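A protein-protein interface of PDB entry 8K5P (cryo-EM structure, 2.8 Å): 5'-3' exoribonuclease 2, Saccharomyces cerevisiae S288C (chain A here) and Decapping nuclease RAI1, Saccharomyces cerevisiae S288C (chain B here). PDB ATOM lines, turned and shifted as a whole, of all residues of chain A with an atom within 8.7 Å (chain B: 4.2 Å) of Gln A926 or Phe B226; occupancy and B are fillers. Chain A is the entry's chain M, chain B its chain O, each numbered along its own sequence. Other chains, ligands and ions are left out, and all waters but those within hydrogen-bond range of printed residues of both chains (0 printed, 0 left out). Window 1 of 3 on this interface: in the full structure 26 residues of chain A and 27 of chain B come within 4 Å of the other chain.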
ATOM      1  N   PRO A 232      24.443  12.037  17.307  1.00  0.00           N
ATOM      2  CA  PRO A 232      24.538  13.469  16.973  1.00  0.00           C
ATOM      3  C   PRO A 232      24.307  13.772  15.503  1.00  0.00           C
ATOM      4  O   PRO A 232      23.771  14.839  15.177  1.00  0.00           O
ATOM      5  CB  PRO A 232      25.967  13.837  17.402  1.00  0.00           C
ATOM      6  CG  PRO A 232      26.408  12.733  18.311  1.00  0.00           C
ATOM      7  CD  PRO A 232      25.707  11.503  17.837  1.00  0.00           C
ATOM      8  N   PRO A 236      17.486  15.216  10.953  1.00  0.00           N
ATOM      9  CA  PRO A 236      16.119  15.486  11.427  1.00  0.00           C
ATOM     10  C   PRO A 236      15.069  15.457  10.329  1.00  0.00           C
ATOM     11  O   PRO A 236      13.872  15.449  10.647  1.00  0.00           O
ATOM     12  CB  PRO A 236      16.227  16.888  12.047  1.00  0.00           C
ATOM     13  CG  PRO A 236      17.702  17.170  12.166  1.00  0.00           C
ATOM     14  CD  PRO A 236      18.357  16.395  11.075  1.00  0.00           C
ATOM     15  N   ASN A 237      15.469  15.441   9.060  1.00  0.00           N
ATOM     16  CA  ASN A 237      14.530  15.478   7.947  1.00  0.00           C
ATOM     17  C   ASN A 237      14.133  14.094   7.451  1.00  0.00           C
ATOM     18  O   ASN A 237      13.390  13.995   6.467  1.00  0.00           O
ATOM     19  CB  ASN A 237      15.122  16.286   6.787  1.00  0.00           C
ATOM     20  CG  ASN A 237      15.578  17.666   7.213  1.00  0.00           C
ATOM     21  OD1 ASN A 237      15.198  18.158   8.276  1.00  0.00           O
ATOM     22  ND2 ASN A 237      16.398  18.301   6.384  1.00  0.00           N
ATOM     23  N   ILE A 874      13.171  19.582  19.349  1.00  0.00           N
ATOM     24  CA  ILE A 874      13.372  19.489  17.910  1.00  0.00           C
ATOM     25  C   ILE A 874      14.852  19.661  17.600  1.00  0.00           C
ATOM     26  O   ILE A 874      15.492  20.622  18.050  1.00  0.00           O
ATOM     27  CB  ILE A 874      12.522  20.538  17.178  1.00  0.00           C
ATOM     28  CG1 ILE A 874      11.042  20.157  17.234  1.00  0.00           C
ATOM     29  CG2 ILE A 874      12.979  20.687  15.734  1.00  0.00           C
ATOM     30  CD1 ILE A 874      10.131  21.135  16.524  1.00  0.00           C
ATOM     31  N   LEU A 875      15.406  18.726  16.833  1.00  0.00           N
ATOM     32  CA  LEU A 875      16.824  18.763  16.508  1.00  0.00           C
ATOM     33  C   LEU A 875      17.147  19.958  15.618  1.00  0.00           C
ATOM     34  O   LEU A 875      16.327  20.405  14.811  1.00  0.00           O
ATOM     35  CB  LEU A 875      17.247  17.467  15.817  1.00  0.00           C
ATOM     36  CG  LEU A 875      17.746  16.345  16.729  1.00  0.00           C
ATOM     37  CD1 LEU A 875      16.581  15.515  17.245  1.00  0.00           C
ATOM     38  CD2 LEU A 875      18.752  15.468  16.001  1.00  0.00           C
ATOM     39  N   ASN A 876      18.360  20.479  15.778  1.00  0.00           N
ATOM     40  CA  ASN A 876      18.808  21.609  14.978  1.00  0.00           C
ATOM     41  C   ASN A 876      18.951  21.208  13.513  1.00  0.00           C
ATOM     42  O   ASN A 876      19.334  20.081  13.187  1.00  0.00           O
ATOM     43  CB  ASN A 876      20.139  22.144  15.508  1.00  0.00           C
ATOM     44  CG  ASN A 876      20.659  23.317  14.702  1.00  0.00           C
ATOM     45  OD1 ASN A 876      19.980  24.334  14.556  1.00  0.00           O
ATOM     46  ND2 ASN A 876      21.870  23.181  14.173  1.00  0.00           N
ATOM     47  N   GLY A 877      18.638  22.150  12.627  1.00  0.00           N
ATOM     48  CA  GLY A 877      18.705  21.909  11.203  1.00  0.00           C
ATOM     49  C   GLY A 877      17.480  21.259  10.601  1.00  0.00           C
ATOM     50  O   GLY A 877      17.496  20.939   9.405  1.00  0.00           O
ATOM     51  N   PHE A 878      16.424  21.048  11.383  1.00  0.00           N
ATOM     52  CA  PHE A 878      15.207  20.447  10.856  1.00  0.00           C
ATOM     53  C   PHE A 878      14.518  21.411   9.898  1.00  0.00           C
ATOM     54  O   PHE A 878      14.325  22.589  10.217  1.00  0.00           O
ATOM     55  CB  PHE A 878      14.270  20.064  12.002  1.00  0.00           C
ATOM     56  CG  PHE A 878      12.812  20.176  11.660  1.00  0.00           C
ATOM     57  CD1 PHE A 878      12.196  19.222  10.868  1.00  0.00           C
ATOM     58  CD2 PHE A 878      12.054  21.232  12.141  1.00  0.00           C
ATOM     59  CE1 PHE A 878      10.855  19.322  10.556  1.00  0.00           C
ATOM     60  CE2 PHE A 878      10.712  21.337  11.831  1.00  0.00           C
ATOM     61  CZ  PHE A 878      10.112  20.380  11.039  1.00  0.00           C
ATOM     62  N   ILE A 879      14.143  20.910   8.728  1.00  0.00           N
ATOM     63  CA  ILE A 879      13.507  21.712   7.687  1.00  0.00           C
ATOM     64  C   ILE A 879      11.999  21.522   7.800  1.00  0.00           C
ATOM     65  O   ILE A 879      11.517  20.391   7.624  1.00  0.00           O
ATOM     66  CB  ILE A 879      14.007  21.323   6.289  1.00  0.00           C
ATOM     67  CG1 ILE A 879      15.505  21.604   6.160  1.00  0.00           C
ATOM     68  CG2 ILE A 879      13.227  22.073   5.221  1.00  0.00           C
ATOM     69  CD1 ILE A 879      15.902  23.004   6.573  1.00  0.00           C
ATOM     70  N   PRO A 880      11.230  22.569   8.088  1.00  0.00           N
ATOM     71  CA  PRO A 880       9.774  22.414   8.173  1.00  0.00           C
ATOM     72  C   PRO A 880       9.168  22.049   6.829  1.00  0.00           C
ATOM     73  O   PRO A 880       9.688  22.398   5.766  1.00  0.00           O
ATOM     74  CB  PRO A 880       9.293  23.793   8.641  1.00  0.00           C
ATOM     75  CG  PRO A 880      10.510  24.468   9.200  1.00  0.00           C
ATOM     76  CD  PRO A 880      11.663  23.937   8.413  1.00  0.00           C
ATOM     77  N   SER A 881       8.049  21.331   6.889  1.00  0.00           N
ATOM     78  CA  SER A 881       7.342  20.938   5.681  1.00  0.00           C
ATOM     79  C   SER A 881       6.679  22.153   5.033  1.00  0.00           C
ATOM     80  O   SER A 881       6.641  23.253   5.594  1.00  0.00           O
ATOM     81  CB  SER A 881       6.300  19.865   5.995  1.00  0.00           C
ATOM     82  OG  SER A 881       5.552  19.527   4.840  1.00  0.00           O
ATOM     83  N   LYS A 922      11.379  21.207   2.484  1.00  0.00           N
ATOM     84  CA  LYS A 922      10.877  22.195   1.527  1.00  0.00           C
ATOM     85  C   LYS A 922      11.594  23.512   1.807  1.00  0.00           C
ATOM     86  O   LYS A 922      11.233  24.236   2.740  1.00  0.00           O
ATOM     87  CB  LYS A 922       9.364  22.349   1.633  1.00  0.00           C
ATOM     88  CG  LYS A 922       8.779  23.392   0.693  1.00  0.00           C
ATOM     89  CD  LYS A 922       9.197  23.136  -0.746  1.00  0.00           C
ATOM     90  CE  LYS A 922       8.428  24.026  -1.711  1.00  0.00           C
ATOM     91  NZ  LYS A 922       9.311  24.589  -2.769  1.00  0.00           N
ATOM     92  N   GLY A 923      12.606  23.816   0.999  1.00  0.00           N
ATOM     93  CA  GLY A 923      13.372  25.034   1.174  1.00  0.00           C
ATOM     94  C   GLY A 923      14.611  24.840   2.021  1.00  0.00           C
ATOM     95  O   GLY A 923      14.579  24.121   3.025  1.00  0.00           O
ATOM     96  N   ILE A 924      15.715  25.474   1.623  1.00  0.00           N
ATOM     97  CA  ILE A 924      16.957  25.352   2.379  1.00  0.00           C
ATOM     98  C   ILE A 924      16.814  26.008   3.750  1.00  0.00           C
ATOM     99  O   ILE A 924      17.233  25.446   4.769  1.00  0.00           O
ATOM    100  CB  ILE A 924      18.127  25.948   1.571  1.00  0.00           C
ATOM    101  CG1 ILE A 924      19.394  26.085   2.424  1.00  0.00           C
ATOM    102  CG2 ILE A 924      17.735  27.286   0.952  1.00  0.00           C
ATOM    103  CD1 ILE A 924      19.843  24.800   3.102  1.00  0.00           C
ATOM    104  N   THR A 925      16.208  27.192   3.801  1.00  0.00           N
ATOM    105  CA  THR A 925      16.055  27.902   5.064  1.00  0.00           C
ATOM    106  C   THR A 925      15.010  27.217   5.935  1.00  0.00           C
ATOM    107  O   THR A 925      13.933  26.847   5.458  1.00  0.00           O
ATOM    108  CB  THR A 925      15.660  29.356   4.811  1.00  0.00           C
ATOM    109  OG1 THR A 925      16.425  29.879   3.717  1.00  0.00           O
ATOM    110  CG2 THR A 925      15.919  30.200   6.050  1.00  0.00           C
ATOM    111  N   GLN A 926      15.331  27.049   7.216  1.00  0.00           N
ATOM    112  CA  GLN A 926      14.429  26.423   8.172  1.00  0.00           C
ATOM    113  C   GLN A 926      13.565  27.428   8.923  1.00  0.00           C
ATOM    114  O   GLN A 926      12.752  27.020   9.758  1.00  0.00           O
ATOM    115  CB  GLN A 926      15.226  25.582   9.175  1.00  0.00           C
ATOM    116  CG  GLN A 926      16.272  26.366   9.948  1.00  0.00           C
ATOM    117  CD  GLN A 926      17.076  25.493  10.889  1.00  0.00           C
ATOM    118  OE1 GLN A 926      16.579  24.491  11.402  1.00  0.00           O
ATOM    119  NE2 GLN A 926      18.328  25.869  11.121  1.00  0.00           N
ATOM    120  N   TYR A 927      13.721  28.721   8.653  1.00  0.00           N
ATOM    121  CA  TYR A 927      12.957  29.767   9.317  1.00  0.00           C
ATOM    122  C   TYR A 927      12.076  30.473   8.298  1.00  0.00           C
ATOM    123  O   TYR A 927      12.554  30.868   7.229  1.00  0.00           O
ATOM    124  CB  TYR A 927      13.882  30.775  10.005  1.00  0.00           C
ATOM    125  CG  TYR A 927      14.768  30.174  11.071  1.00  0.00           C
ATOM    126  CD1 TYR A 927      14.258  29.836  12.317  1.00  0.00           C
ATOM    127  CD2 TYR A 927      16.116  29.946  10.831  1.00  0.00           C
ATOM    128  CE1 TYR A 927      15.065  29.288  13.294  1.00  0.00           C
ATOM    129  CE2 TYR A 927      16.932  29.399  11.803  1.00  0.00           C
ATOM    130  CZ  TYR A 927      16.401  29.071  13.031  1.00  0.00           C
ATOM    131  OH  TYR A 927      17.211  28.525  14.001  1.00  0.00           O
ATOM    132  N   LYS A 928      10.799  30.628   8.629  1.00  0.00           N
ATOM    133  CA  LYS A 928       9.891  31.344   7.747  1.00  0.00           C
ATOM    134  C   LYS A 928      10.257  32.827   7.715  1.00  0.00           C
ATOM    135  O   LYS A 928      10.684  33.385   8.731  1.00  0.00           O
ATOM    136  CB  LYS A 928       8.443  31.167   8.205  1.00  0.00           C
ATOM    137  CG  LYS A 928       8.209  31.487   9.671  1.00  0.00           C
ATOM    138  CD  LYS A 928       7.179  30.551  10.282  1.00  0.00           C
ATOM    139  CE  LYS A 928       6.596  31.129  11.561  1.00  0.00           C
ATOM    140  NZ  LYS A 928       6.214  32.560  11.400  1.00  0.00           N
ATOM    141  N   PRO A 929      10.110  33.491   6.568  1.00  0.00           N
ATOM    142  CA  PRO A 929      10.488  34.907   6.462  1.00  0.00           C
ATOM    143  C   PRO A 929       9.466  35.809   7.138  1.00  0.00           C
ATOM    144  O   PRO A 929       8.337  35.966   6.661  1.00  0.00           O
ATOM    145  CB  PRO A 929      10.543  35.137   4.944  1.00  0.00           C
ATOM    146  CG  PRO A 929       9.602  34.133   4.378  1.00  0.00           C
ATOM    147  CD  PRO A 929       9.659  32.932   5.280  1.00  0.00           C
ATOM    148  N   ARG A 930       9.863  36.407   8.258  1.00  0.00           N
ATOM    149  CA  ARG A 930       9.047  37.381   8.974  1.00  0.00           C
ATOM    150  C   ARG A 930       9.823  38.688   9.052  1.00  0.00           C
ATOM    151  O   ARG A 930      10.928  38.719   9.604  1.00  0.00           O
ATOM    152  CB  ARG A 930       8.687  36.882  10.375  1.00  0.00           C
ATOM    153  CG  ARG A 930       8.793  35.377  10.552  1.00  0.00           C
ATOM    154  CD  ARG A 930       8.846  35.001  12.024  1.00  0.00           C
ATOM    155  NE  ARG A 930       9.011  33.565  12.217  1.00  0.00           N
ATOM    156  CZ  ARG A 930      10.181  32.944  12.252  1.00  0.00           C
ATOM    157  NH1 ARG A 930      11.319  33.604  12.110  1.00  0.00           N
ATOM    158  NH2 ARG A 930      10.211  31.627  12.433  1.00  0.00           N
ATOM    159  N   ARG A 935      16.196  38.571   1.322  1.00  0.00           N
ATOM    160  CA  ARG A 935      15.377  37.484   0.794  1.00  0.00           C
ATOM    161  C   ARG A 935      13.914  37.668   1.174  1.00  0.00           C
ATOM    162  O   ARG A 935      13.018  37.483   0.342  1.00  0.00           O
ATOM    163  CB  ARG A 935      15.902  36.139   1.298  1.00  0.00           C
ATOM    164  CG  ARG A 935      15.220  34.935   0.671  1.00  0.00           C
ATOM    165  CD  ARG A 935      16.112  33.706   0.720  1.00  0.00           C
ATOM    166  NE  ARG A 935      16.857  33.621   1.970  1.00  0.00           N
ATOM    167  CZ  ARG A 935      18.128  33.252   2.061  1.00  0.00           C
ATOM    168  NH1 ARG A 935      18.831  32.924   0.990  1.00  0.00           N
ATOM    169  NH2 ARG A 935      18.707  33.210   3.258  1.00  0.00           N
ATOM    170  N   TYR B  46      25.274  25.479  17.848  1.00  0.00           N
ATOM    171  CA  TYR B  46      24.120  26.308  17.535  1.00  0.00           C
ATOM    172  C   TYR B  46      22.826  25.521  17.695  1.00  0.00           C
ATOM    173  O   TYR B  46      22.736  24.356  17.300  1.00  0.00           O
ATOM    174  CB  TYR B  46      24.227  26.852  16.110  1.00  0.00           C
ATOM    175  CG  TYR B  46      23.042  27.686  15.677  1.00  0.00           C
ATOM    176  CD1 TYR B  46      22.910  29.005  16.089  1.00  0.00           C
ATOM    177  CD2 TYR B  46      22.057  27.154  14.856  1.00  0.00           C
ATOM    178  CE1 TYR B  46      21.830  29.772  15.696  1.00  0.00           C
ATOM    179  CE2 TYR B  46      20.973  27.912  14.458  1.00  0.00           C
ATOM    180  CZ  TYR B  46      20.865  29.220  14.880  1.00  0.00           C
ATOM    181  OH  TYR B  46      19.787  29.979  14.486  1.00  0.00           O
ATOM    182  N   ILE B 225      29.438  25.632  15.715  1.00  0.00           N
ATOM    183  CA  ILE B 225      29.462  24.423  14.900  1.00  0.00           C
ATOM    184  C   ILE B 225      28.019  24.042  14.598  1.00  0.00           C
ATOM    185  O   ILE B 225      27.186  23.972  15.510  1.00  0.00           O
ATOM    186  CB  ILE B 225      30.219  23.277  15.602  1.00  0.00           C
ATOM    187  CG1 ILE B 225      30.102  21.974  14.809  1.00  0.00           C
ATOM    188  CG2 ILE B 225      29.740  23.097  17.028  1.00  0.00           C
ATOM    189  CD1 ILE B 225      30.622  22.073  13.400  1.00  0.00           C
ATOM    190  N   PHE B 226      27.720  23.817  13.319  1.00  0.00           N
ATOM    191  CA  PHE B 226      26.344  23.641  12.875  1.00  0.00           C
ATOM    192  C   PHE B 226      25.915  22.186  12.749  1.00  0.00           C
ATOM    193  O   PHE B 226      24.709  21.913  12.768  1.00  0.00           O
ATOM    194  CB  PHE B 226      26.133  24.338  11.525  1.00  0.00           C
ATOM    195  CG  PHE B 226      24.701  24.691  11.240  1.00  0.00           C
ATOM    196  CD1 PHE B 226      24.103  25.773  11.864  1.00  0.00           C
ATOM    197  CD2 PHE B 226      23.954  23.940  10.348  1.00  0.00           C
ATOM    198  CE1 PHE B 226      22.785  26.099  11.604  1.00  0.00           C
ATOM    199  CE2 PHE B 226      22.637  24.261  10.084  1.00  0.00           C
ATOM    200  CZ  PHE B 226      22.052  25.342  10.712  1.00  0.00           C
ATOM    201  N   ASP B 227      26.853  21.252  12.624  1.00  0.00           N
ATOM    202  CA  ASP B 227      26.517  19.851  12.404  1.00  0.00           C
ATOM    203  C   ASP B 227      27.389  18.993  13.313  1.00  0.00           C
ATOM    204  O   ASP B 227      28.064  19.494  14.217  1.00  0.00           O
ATOM    205  CB  ASP B 227      26.682  19.481  10.924  1.00  0.00           C
ATOM    206  CG  ASP B 227      25.757  20.270  10.018  1.00  0.00           C
ATOM    207  OD1 ASP B 227      26.089  21.430   9.694  1.00  0.00           O
ATOM    208  OD2 ASP B 227      24.699  19.733   9.631  1.00  0.00           O
ATOM    209  N   HIS B 238      31.920  21.921   8.236  1.00  0.00           N
ATOM    210  CA  HIS B 238      30.820  21.864   9.189  1.00  0.00           C
ATOM    211  C   HIS B 238      30.680  23.128  10.028  1.00  0.00           C
ATOM    212  O   HIS B 238      29.617  23.340  10.622  1.00  0.00           O
ATOM    213  CB  HIS B 238      30.991  20.662  10.127  1.00  0.00           C
ATOM    214  CG  HIS B 238      30.958  19.335   9.432  1.00  0.00           C
ATOM    215  ND1 HIS B 238      30.700  18.156  10.097  1.00  0.00           N
ATOM    216  CD2 HIS B 238      31.148  19.001   8.134  1.00  0.00           C
ATOM    217  CE1 HIS B 238      30.734  17.152   9.238  1.00  0.00           C
ATOM    218  NE2 HIS B 238      31.004  17.639   8.040  1.00  0.00           N
ATOM    219  N   ALA B 240      30.321  27.116  11.268  1.00  0.00           N
ATOM    220  CA  ALA B 240      29.410  28.191  10.906  1.00  0.00           C
ATOM    221  C   ALA B 240      29.738  29.419  11.742  1.00  0.00           C
ATOM    222  O   ALA B 240      30.359  29.325  12.804  1.00  0.00           O
ATOM    223  CB  ALA B 240      27.946  27.781  11.102  1.00  0.00           C
ATOM    224  N   ARG B 275      28.801  28.429   6.106  1.00  0.00           N
ATOM    225  CA  ARG B 275      27.504  28.888   6.588  1.00  0.00           C
ATOM    226  C   ARG B 275      27.656  30.227   7.294  1.00  0.00           C
ATOM    227  O   ARG B 275      28.545  30.395   8.134  1.00  0.00           O
ATOM    228  CB  ARG B 275      26.876  27.861   7.534  1.00  0.00           C
ATOM    229  CG  ARG B 275      26.786  26.459   6.955  1.00  0.00           C
ATOM    230  CD  ARG B 275      26.388  25.449   8.019  1.00  0.00           C
ATOM    231  NE  ARG B 275      26.084  24.142   7.447  1.00  0.00           N
ATOM    232  CZ  ARG B 275      24.905  23.799   6.948  1.00  0.00           C
ATOM    233  NH1 ARG B 275      23.888  24.645   6.933  1.00  0.00           N
ATOM    234  NH2 ARG B 275      24.741  22.577   6.451  1.00  0.00           N
ATOM    235  N   ILE B 277      25.271  33.091   9.408  1.00  0.00           N
ATOM    236  CA  ILE B 277      24.009  33.301  10.107  1.00  0.00           C
ATOM    237  C   ILE B 277      23.938  34.757  10.542  1.00  0.00           C
ATOM    238  O   ILE B 277      24.898  35.287  11.114  1.00  0.00           O
ATOM    239  CB  ILE B 277      23.866  32.360  11.317  1.00  0.00           C
ATOM    240  CG1 ILE B 277      24.053  30.904  10.886  1.00  0.00           C
ATOM    241  CG2 ILE B 277      22.512  32.548  11.983  1.00  0.00           C
ATOM    242  CD1 ILE B 277      23.947  29.911  12.022  1.00  0.00           C
ATOM    243  N   GLU B 292      19.904  32.068   7.653  1.00  0.00           N
ATOM    244  CA  GLU B 292      21.225  31.552   7.319  1.00  0.00           C
ATOM    245  C   GLU B 292      21.548  31.850   5.862  1.00  0.00           C
ATOM    246  O   GLU B 292      20.667  31.814   4.997  1.00  0.00           O
ATOM    247  CB  GLU B 292      21.304  30.046   7.574  1.00  0.00           C
ATOM    248  CG  GLU B 292      19.989  29.312   7.380  1.00  0.00           C
ATOM    249  CD  GLU B 292      19.291  29.018   8.692  1.00  0.00           C
ATOM    250  OE1 GLU B 292      18.952  29.981   9.412  1.00  0.00           O
ATOM    251  OE2 GLU B 292      19.081  27.828   9.002  1.00  0.00           O
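N of Gly A877 is in hydrogen-bond range of OE1 of Gln A926, at 3.3 Å. The backbone carbonyl oxygen of Phe A878 sits close to the side-chain amide oxygen of Gln A926, at 3.2 Å. The backbone NH (N) of Tyr B46 sits at hydrogen-bond distance from the backbone carbonyl oxygen (O) of Ile B225. The backbone carbonyl oxygen of His B238 is in hydrogen-bond range of the backbone NH of Phe B226 (3.3 Å).
The side-chain amide nitrogen (ND2) of Asn A876 lies within hydrogen-bond range of the backbone carbonyl oxygen (O) of Tyr B46 (3.5 Å). The backbone carbonyl oxygen (O) of Phe B226 sits at hydrogen-bond distance from the side-chain amide nitrogen (ND2) of Asn A876 (3.4 Å). The side-chain amide nitrogen (NE2) of Gln A926 is in hydrogen-bond range of the side-chain carboxylate (OE2) of Glu B292. OH of Tyr B46 is in hydrogen-bond range of OH of Tyr A927 (3.0 Å). The backbone carbonyl oxygen (O) of Glu B292 lies within hydrogen-bond range of the guanidinium group (NH2) of Arg A935, 3.0 Å away.
NE2 of Gln A926 touches CZ of Phe B226 (3.8 Å). Glu B292 touches Tyr A927.
Gln A926 touches just these residues of chain B: Phe B226 (3.8 Å) and Glu B292 (3.0 Å). Printed residues of chain A within 4 Å of Phe B226: Asn A876 and Gln A926. No residue of chain A comes within 4 Å of Ile B225. Printed residues of chain B within 4 Å of Arg A935: Glu B292 (3.0 Å). Of the printed residues of chain A, Glu B292 touches Gln A926, Tyr A927 and Arg A935. Printed residues of chain B within 4 Å of Asn A876: Tyr B46 (3.5 Å) and Phe B226 (3.4 Å). Of the printed residues of chain B, Tyr A927 touches Tyr B46 and Glu B292. Ile A874 touches none of the printed residues of chain B. Thr A925 touches none of the printed residues of chain B. The nearest printed residue of chain A that does not touch Glu B292 is Thr A925 (4.4 Å).
Hydrophobic or aromatic side chains of chain B within 4 Å of the printed part of chain A: Tyr B46 and Phe B226. Among the printed residues, no Asp or Glu carboxylate lies within 4 Å of a Lys or Arg side-chain nitrogen of the other chain.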
